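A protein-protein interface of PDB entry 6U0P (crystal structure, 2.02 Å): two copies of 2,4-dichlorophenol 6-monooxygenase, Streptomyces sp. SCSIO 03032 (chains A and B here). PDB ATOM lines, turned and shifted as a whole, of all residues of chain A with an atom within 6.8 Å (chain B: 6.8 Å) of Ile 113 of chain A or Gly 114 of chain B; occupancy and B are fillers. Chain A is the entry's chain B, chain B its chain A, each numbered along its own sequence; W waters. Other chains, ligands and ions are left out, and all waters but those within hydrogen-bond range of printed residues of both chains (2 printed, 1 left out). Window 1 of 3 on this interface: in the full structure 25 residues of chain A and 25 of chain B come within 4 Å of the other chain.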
ATOM      1  N   GLY A 107     -24.939  -4.403 -31.351  1.00  0.00           N
ATOM      2  CA  GLY A 107     -25.004  -3.138 -30.616  1.00  0.00           C
ATOM      3  C   GLY A 107     -24.101  -2.051 -31.221  1.00  0.00           C
ATOM      4  O   GLY A 107     -23.900  -1.070 -30.552  1.00  0.00           O
ATOM      5  N   ASN A 108     -23.677  -2.174 -32.478  1.00  0.00           N
ATOM      6  CA  ASN A 108     -22.820  -1.153 -33.134  1.00  0.00           C
ATOM      7  C   ASN A 108     -23.649  -0.034 -33.767  1.00  0.00           C
ATOM      8  O   ASN A 108     -23.097   1.065 -33.937  1.00  0.00           O
ATOM      9  CB  ASN A 108     -21.912  -1.786 -34.167  1.00  0.00           C
ATOM     10  CG  ASN A 108     -20.729  -2.459 -33.508  1.00  0.00           C
ATOM     11  OD1 ASN A 108     -19.771  -1.779 -33.164  1.00  0.00           O
ATOM     12  ND2 ASN A 108     -20.762  -3.770 -33.354  1.00  0.00           N
ATOM     13  N   GLY A 109     -24.911  -0.284 -34.117  1.00  0.00           N
ATOM     14  CA  GLY A 109     -25.766   0.755 -34.715  1.00  0.00           C
ATOM     15  C   GLY A 109     -26.033   1.863 -33.710  1.00  0.00           C
ATOM     16  O   GLY A 109     -26.226   1.584 -32.540  1.00  0.00           O
ATOM     17  N   PRO A 110     -26.077   3.152 -34.125  1.00  0.00           N
ATOM     18  CA  PRO A 110     -26.387   4.257 -33.211  1.00  0.00           C
ATOM     19  C   PRO A 110     -27.651   4.110 -32.361  1.00  0.00           C
ATOM     20  O   PRO A 110     -27.758   4.657 -31.242  1.00  0.00           O
ATOM     21  CB  PRO A 110     -26.628   5.429 -34.183  1.00  0.00           C
ATOM     22  CG  PRO A 110     -25.724   5.108 -35.338  1.00  0.00           C
ATOM     23  CD  PRO A 110     -25.833   3.611 -35.505  1.00  0.00           C
ATOM     24  N   ASP A 111     -28.643   3.388 -32.856  1.00  0.00           N
ATOM     25  CA  ASP A 111     -29.891   3.255 -32.053  1.00  0.00           C
ATOM     26  C   ASP A 111     -29.701   2.200 -30.935  1.00  0.00           C
ATOM     27  O   ASP A 111     -30.430   2.287 -29.967  1.00  0.00           O
ATOM     28  CB  ASP A 111     -31.085   3.077 -32.980  1.00  0.00           C
ATOM     29  CG  ASP A 111     -31.227   1.659 -33.451  1.00  0.00           C
ATOM     30  OD1 ASP A 111     -30.215   1.107 -33.954  1.00  0.00           O
ATOM     31  OD2 ASP A 111     -32.334   1.100 -33.270  1.00  0.00           O
ATOM     32  N   ARG A 112     -28.693   1.313 -30.979  1.00  0.00           N
ATOM     33  CA  ARG A 112     -28.501   0.260 -29.934  1.00  0.00           C
ATOM     34  C   ARG A 112     -27.210   0.493 -29.121  1.00  0.00           C
ATOM     35  O   ARG A 112     -27.127  -0.037 -27.997  1.00  0.00           O
ATOM     36  CB  ARG A 112     -28.486  -1.136 -30.571  1.00  0.00           C
ATOM     37  CG  ARG A 112     -29.698  -1.496 -31.430  1.00  0.00           C
ATOM     38  CD  ARG A 112     -31.033  -1.273 -30.732  1.00  0.00           C
ATOM     39  NE  ARG A 112     -31.093  -1.856 -29.389  1.00  0.00           N
ATOM     40  CZ  ARG A 112     -31.336  -3.147 -29.127  1.00  0.00           C
ATOM     41  NH1 ARG A 112     -31.550  -4.026 -30.103  1.00  0.00           N
ATOM     42  NH2 ARG A 112     -31.305  -3.549 -27.883  1.00  0.00           N
ATOM     43  N   ILE A 113     -26.240   1.276 -29.621  1.00  0.00           N
ATOM     44  CA  ILE A 113     -24.879   1.400 -29.002  1.00  0.00           C
ATOM     45  C   ILE A 113     -24.971   1.877 -27.553  1.00  0.00           C
ATOM     46  O   ILE A 113     -24.259   1.313 -26.726  1.00  0.00           O
ATOM     47  CB  ILE A 113     -23.924   2.289 -29.829  1.00  0.00           C
ATOM     48  CG1 ILE A 113     -22.512   2.207 -29.254  1.00  0.00           C
ATOM     49  CG2 ILE A 113     -24.400   3.713 -29.918  1.00  0.00           C
ATOM     50  CD1 ILE A 113     -21.451   2.519 -30.251  1.00  0.00           C
ATOM     51  N   GLY A 114     -25.800   2.874 -27.263  1.00  0.00           N
ATOM     52  CA  GLY A 114     -26.015   3.410 -25.909  1.00  0.00           C
ATOM     53  C   GLY A 114     -26.463   2.309 -24.953  1.00  0.00           C
ATOM     54  O   GLY A 114     -25.834   2.149 -23.864  1.00  0.00           O
ATOM     55  N   GLU A 115     -27.469   1.514 -25.359  1.00  0.00           N
ATOM     56  CA  GLU A 115     -28.025   0.435 -24.499  1.00  0.00           C
ATOM     57  C   GLU A 115     -26.927  -0.612 -24.282  1.00  0.00           C
ATOM     58  O   GLU A 115     -26.815  -1.088 -23.145  1.00  0.00           O
ATOM     59  CB  GLU A 115     -29.276  -0.207 -25.109  1.00  0.00           C
ATOM     60  CG  GLU A 115     -30.435   0.768 -25.231  1.00  0.00           C
ATOM     61  CD  GLU A 115     -31.580   0.535 -26.241  1.00  0.00           C
ATOM     62  OE1 GLU A 115     -31.372   0.068 -27.426  1.00  0.00           O
ATOM     63  OE2 GLU A 115     -32.710   0.916 -25.852  1.00  0.00           O
ATOM     64  N   TYR A 116     -26.149  -0.951 -25.309  1.00  0.00           N
ATOM     65  CA  TYR A 116     -25.122  -2.025 -25.201  1.00  0.00           C
ATOM     66  C   TYR A 116     -23.995  -1.552 -24.276  1.00  0.00           C
ATOM     67  O   TYR A 116     -23.566  -2.355 -23.416  1.00  0.00           O
ATOM     68  CB  TYR A 116     -24.588  -2.485 -26.559  1.00  0.00           C
ATOM     69  CG  TYR A 116     -25.374  -3.596 -27.209  1.00  0.00           C
ATOM     70  CD1 TYR A 116     -24.806  -4.828 -27.488  1.00  0.00           C
ATOM     71  CD2 TYR A 116     -26.714  -3.425 -27.537  1.00  0.00           C
ATOM     72  CE1 TYR A 116     -25.526  -5.816 -28.153  1.00  0.00           C
ATOM     73  CE2 TYR A 116     -27.449  -4.423 -28.162  1.00  0.00           C
ATOM     74  CZ  TYR A 116     -26.867  -5.643 -28.429  1.00  0.00           C
ATOM     75  OH  TYR A 116     -27.587  -6.624 -29.052  1.00  0.00           O
ATOM     76  N   ARG A 117     -23.634  -0.266 -24.326  1.00  0.00           N
ATOM     77  CA  ARG A 117     -22.571   0.284 -23.433  1.00  0.00           C
ATOM     78  C   ARG A 117     -23.061   0.367 -21.996  1.00  0.00           C
ATOM     79  O   ARG A 117     -22.297   0.041 -21.123  1.00  0.00           O
ATOM     80  CB  ARG A 117     -22.138   1.659 -23.920  1.00  0.00           C
ATOM     81  CG  ARG A 117     -21.630   1.599 -25.347  1.00  0.00           C
ATOM     82  CD  ARG A 117     -20.149   1.476 -25.381  1.00  0.00           C
ATOM     83  NE  ARG A 117     -19.611   2.809 -25.270  1.00  0.00           N
ATOM     84  CZ  ARG A 117     -18.817   3.378 -26.158  1.00  0.00           C
ATOM     85  NH1 ARG A 117     -18.455   2.742 -27.265  1.00  0.00           N
ATOM     86  NH2 ARG A 117     -18.421   4.612 -25.935  1.00  0.00           N
ATOM     87  N   ALA A 118     -24.301   0.767 -21.732  1.00  0.00           N
ATOM     88  CA  ALA A 118     -24.797   0.886 -20.340  1.00  0.00           C
ATOM     89  C   ALA A 118     -24.990  -0.495 -19.673  1.00  0.00           C
ATOM     90  O   ALA A 118     -25.089  -0.546 -18.388  1.00  0.00           O
ATOM     91  CB  ALA A 118     -26.120   1.644 -20.316  1.00  0.00           C
ATOM     92  N   GLY B 107     -21.109  13.909 -25.547  1.00  0.00           N
ATOM     93  CA  GLY B 107     -21.820  12.749 -26.097  1.00  0.00           C
ATOM     94  C   GLY B 107     -21.118  11.428 -25.837  1.00  0.00           C
ATOM     95  O   GLY B 107     -21.405  10.450 -26.603  1.00  0.00           O
ATOM     96  N   GLY B 109     -21.405   9.760 -22.834  1.00  0.00           N
ATOM     97  CA  GLY B 109     -22.236   8.976 -21.902  1.00  0.00           C
ATOM     98  C   GLY B 109     -23.175   8.061 -22.676  1.00  0.00           C
ATOM     99  O   GLY B 109     -23.644   8.412 -23.769  1.00  0.00           O
ATOM    100  N   PRO B 110     -23.456   6.837 -22.165  1.00  0.00           N
ATOM    101  CA  PRO B 110     -24.389   5.936 -22.855  1.00  0.00           C
ATOM    102  C   PRO B 110     -25.748   6.518 -23.288  1.00  0.00           C
ATOM    103  O   PRO B 110     -26.302   6.134 -24.335  1.00  0.00           O
ATOM    104  CB  PRO B 110     -24.576   4.828 -21.807  1.00  0.00           C
ATOM    105  CG  PRO B 110     -23.282   4.800 -21.035  1.00  0.00           C
ATOM    106  CD  PRO B 110     -22.854   6.244 -20.956  1.00  0.00           C
ATOM    107  N   ASP B 111     -26.317   7.427 -22.508  1.00  0.00           N
ATOM    108  CA  ASP B 111     -27.621   8.045 -22.867  1.00  0.00           C
ATOM    109  C   ASP B 111     -27.501   9.034 -24.048  1.00  0.00           C
ATOM    110  O   ASP B 111     -28.564   9.367 -24.620  1.00  0.00           O
ATOM    111  CB  ASP B 111     -28.279   8.682 -21.653  1.00  0.00           C
ATOM    112  CG  ASP B 111     -27.451   9.806 -21.087  1.00  0.00           C
ATOM    113  OD1 ASP B 111     -26.218   9.593 -20.908  1.00  0.00           O
ATOM    114  OD2 ASP B 111     -28.037  10.897 -20.860  1.00  0.00           O
ATOM    115  N   ARG B 112     -26.301   9.462 -24.495  1.00  0.00           N
ATOM    116  CA  ARG B 112     -26.197  10.484 -25.586  1.00  0.00           C
ATOM    117  C   ARG B 112     -25.416   9.932 -26.785  1.00  0.00           C
ATOM    118  O   ARG B 112     -25.525  10.506 -27.912  1.00  0.00           O
ATOM    119  CB  ARG B 112     -25.575  11.782 -25.038  1.00  0.00           C
ATOM    120  CG  ARG B 112     -26.272  12.350 -23.798  1.00  0.00           C
ATOM    121  CD  ARG B 112     -27.775  12.713 -23.906  1.00  0.00           C
ATOM    122  NE  ARG B 112     -28.099  13.393 -25.162  1.00  0.00           N
ATOM    123  CZ  ARG B 112     -27.984  14.706 -25.397  1.00  0.00           C
ATOM    124  NH1 ARG B 112     -27.643  15.548 -24.443  1.00  0.00           N
ATOM    125  NH2 ARG B 112     -28.250  15.162 -26.603  1.00  0.00           N
ATOM    126  N   ILE B 113     -24.656   8.856 -26.590  1.00  0.00           N
ATOM    127  CA  ILE B 113     -23.633   8.425 -27.568  1.00  0.00           C
ATOM    128  C   ILE B 113     -24.323   8.096 -28.879  1.00  0.00           C
ATOM    129  O   ILE B 113     -23.797   8.484 -29.954  1.00  0.00           O
ATOM    130  CB  ILE B 113     -22.727   7.288 -27.061  1.00  0.00           C
ATOM    131  CG1 ILE B 113     -21.642   7.047 -28.110  1.00  0.00           C
ATOM    132  CG2 ILE B 113     -23.508   6.005 -26.717  1.00  0.00           C
ATOM    133  CD1 ILE B 113     -20.457   6.249 -27.601  1.00  0.00           C
ATOM    134  N   GLY B 114     -25.493   7.470 -28.824  1.00  0.00           N
ATOM    135  CA  GLY B 114     -26.176   7.055 -30.051  1.00  0.00           C
ATOM    136  C   GLY B 114     -26.643   8.256 -30.840  1.00  0.00           C
ATOM    137  O   GLY B 114     -26.448   8.257 -32.043  1.00  0.00           O
ATOM    138  N   GLU B 115     -27.256   9.238 -30.181  1.00  0.00           N
ATOM    139  CA  GLU B 115     -27.715  10.483 -30.850  1.00  0.00           C
ATOM    140  C   GLU B 115     -26.469  11.198 -31.435  1.00  0.00           C
ATOM    141  O   GLU B 115     -26.531  11.710 -32.616  1.00  0.00           O
ATOM    142  CB  GLU B 115     -28.508  11.384 -29.889  1.00  0.00           C
ATOM    143  CG  GLU B 115     -29.781  10.754 -29.318  1.00  0.00           C
ATOM    144  CD  GLU B 115     -30.362  11.274 -27.975  1.00  0.00           C
ATOM    145  OE1 GLU B 115     -29.609  11.514 -26.950  1.00  0.00           O
ATOM    146  OE2 GLU B 115     -31.625  11.405 -27.916  1.00  0.00           O
ATOM    147  N   TYR B 116     -25.330  11.207 -30.729  1.00  0.00           N
ATOM    148  CA  TYR B 116     -24.137  11.935 -31.274  1.00  0.00           C
ATOM    149  C   TYR B 116     -23.625  11.269 -32.542  1.00  0.00           C
ATOM    150  O   TYR B 116     -23.354  11.974 -33.551  1.00  0.00           O
ATOM    151  CB  TYR B 116     -23.048  12.138 -30.232  1.00  0.00           C
ATOM    152  CG  TYR B 116     -23.234  13.359 -29.377  1.00  0.00           C
ATOM    153  CD1 TYR B 116     -22.255  14.350 -29.334  1.00  0.00           C
ATOM    154  CD2 TYR B 116     -24.391  13.549 -28.635  1.00  0.00           C
ATOM    155  CE1 TYR B 116     -22.400  15.465 -28.538  1.00  0.00           C
ATOM    156  CE2 TYR B 116     -24.562  14.674 -27.847  1.00  0.00           C
ATOM    157  CZ  TYR B 116     -23.560  15.641 -27.800  1.00  0.00           C
ATOM    158  OH  TYR B 116     -23.696  16.770 -27.032  1.00  0.00           O
ATOM    159  N   ARG B 117     -23.560   9.935 -32.570  1.00  0.00           N
ATOM    160  CA  ARG B 117     -23.020   9.211 -33.736  1.00  0.00           C
ATOM    161  C   ARG B 117     -23.993   9.273 -34.907  1.00  0.00           C
ATOM    162  O   ARG B 117     -23.513   9.254 -36.059  1.00  0.00           O
ATOM    163  CB  ARG B 117     -22.741   7.748 -33.409  1.00  0.00           C
ATOM    164  CG  ARG B 117     -22.102   7.571 -32.043  1.00  0.00           C
ATOM    165  CD  ARG B 117     -20.677   7.179 -32.090  1.00  0.00           C
ATOM    166  NE  ARG B 117     -20.615   5.818 -32.554  1.00  0.00           N
ATOM    167  CZ  ARG B 117     -19.717   4.929 -32.151  1.00  0.00           C
ATOM    168  NH1 ARG B 117     -18.808   5.232 -31.232  1.00  0.00           N
ATOM    169  NH2 ARG B 117     -19.753   3.720 -32.679  1.00  0.00           N
ATOM    170  N   ALA B 118     -25.302   9.265 -34.636  1.00  0.00           N
ATOM    171  CA  ALA B 118     -26.334   9.405 -35.688  1.00  0.00           C
ATOM    172  C   ALA B 118     -26.285  10.796 -36.354  1.00  0.00           C
ATOM    173  O   ALA B 118     -26.757  10.943 -37.472  1.00  0.00           O
ATOM    174  CB  ALA B 118     -27.696   9.167 -35.096  1.00  0.00           C
ATOM    175  N   ALA B 119     -25.847  11.814 -35.646  1.00  0.00           N
ATOM    176  CA  ALA B 119     -26.148  13.217 -36.003  1.00  0.00           C
ATOM    177  C   ALA B 119     -25.164  13.772 -37.040  1.00  0.00           C
ATOM    178  O   ALA B 119     -25.552  14.693 -37.764  1.00  0.00           O
ATOM    179  CB  ALA B 119     -26.182  14.044 -34.744  1.00  0.00           C
HETATM  180  O   HOH W   1     -22.895   3.908 -33.876  1.00  0.00           O
HETATM  181  O   HOH W   2     -16.348   3.624 -29.701  1.00  0.00           O
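Water W1 lies within hydrogen-bond range of the backbone carbonyl oxygen of Asn 108 of chain A (2.9 Å) and the guanidinium group of Arg 117 of chain B (3.3 Å). Water W2 bridges the guanidinium group (NH1) of Arg 117 of chain B (3.3 Å) and the guanidinium group (NH1) of Arg 117 of chain A (3.3 Å).
Of the 12 printed residues of chain B, 5 touch a printed residue of chain A. Hydrophobic or aromatic side chains of chain B that line the printed part of chain A: Pro 110, Ile 113 and Ala 118. Of the 12 printed residues of chain A, 5 touch a printed residue of chain B. Among the printed residues, 8 pairs touch across the chains. Among the printed residues, no Asp or Glu carboxylate lies within 4 Å of a Lys or Arg side-chain nitrogen of the other chain.
Pro 110 of chain A touches Gly 114 of chain B, and with the chains exchanged Gly 114 of chain A touches Pro 110 of chain B. Pro 110 of chain A touches Ala 118 of chain B, and with the chains exchanged Ala 118 of chain A touches Pro 110 of chain B. Ile 113 of chain A touches Gly 114 of chain B, and with the chains exchanged Gly 114 of chain A touches Ile 113 of chain B. Ile 113 of chain A touches Arg 117 of chain B, and with the chains exchanged Arg 117 of chain A touches Ile 113 of chain B. Positions printed for both chains: 107, 109, 110, 111, 112, 113, 114, 115, 116, 117 and 118. Of the 8 pairs that touch across the chains among the printed residues, 8 have their exchanged pair printed and touching as well.
Of chain B, only Gly 114 and Arg 117 come within 4 Å of Ile 113 of chain A. Of chain A, only Pro 110 (3.1 Å) and Ile 113 (3.8 Å) come within 4 Å of Gly 114 of chain B. Printed residues of chain B within 4 Å of Arg 117 of chain A: Ile 113. Of the printed residues of chain A, Pro 110 of chain B touches Gly 114 (3.2 Å) and Ala 118 (3.8 Å). Of the printed residues of chain B, Pro 110 of chain A touches Gly 114 (3.1 Å) and Ala 118 (3.99 Å). Printed residues of chain B within 4 Å of Gly 114 of chain A: Pro 110 (3.2 Å) and Ile 113 (3.7 Å). Of the printed residues of chain A, Ile 113 of chain B touches Gly 114 (3.7 Å) and Arg 117 (3.1 Å). Asp 111 of chain B touches none of the printed residues of chain A. Glu 115 of chain B touches none of the printed residues of chain A. The nearest residue of chain B that does not touch Ile 113 of chain A is Ile 113 of chain B (4.04 Å). The nearest residue of chain A that does not touch Gly 114 of chain B is Gly 114 of chain A (4.9 Å). The nearest printed residue of chain B that does not touch Arg 117 of chain A is Pro 110 of chain B (4.4 Å).
The backbone carbonyl oxygen (O) of Gly 107 of chain A lies close to the backbone NH (N) of Ile 113 of chain A (3.4 Å).
O of Pro 110 of chain A touches CA of Gly 114 of chain B, at 3.1 Å. CB of Pro 110 of chain A touches CB of Ala 118 of chain B, at 3.99 Å. CG2 of Ile 113 of chain A touches CA of Gly 114 of chain B, at 3.8 Å. Ile 113 of chain A touches Arg 117 of chain B (CD1 to NH2, 3.2 Å). CA of Gly 114 of chain A touches O of Pro 110 of chain B (3.2 Å). Gly 114 of chain A touches Ile 113 of chain B (CA to CG2, 3.7 Å). Arg 117 of chain A touches Ile 113 of chain B (NH2 to CD1, 3.1 Å). CB of Pro 110 of chain B touches CB of Ala 118 of chain A, at 3.8 Å.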
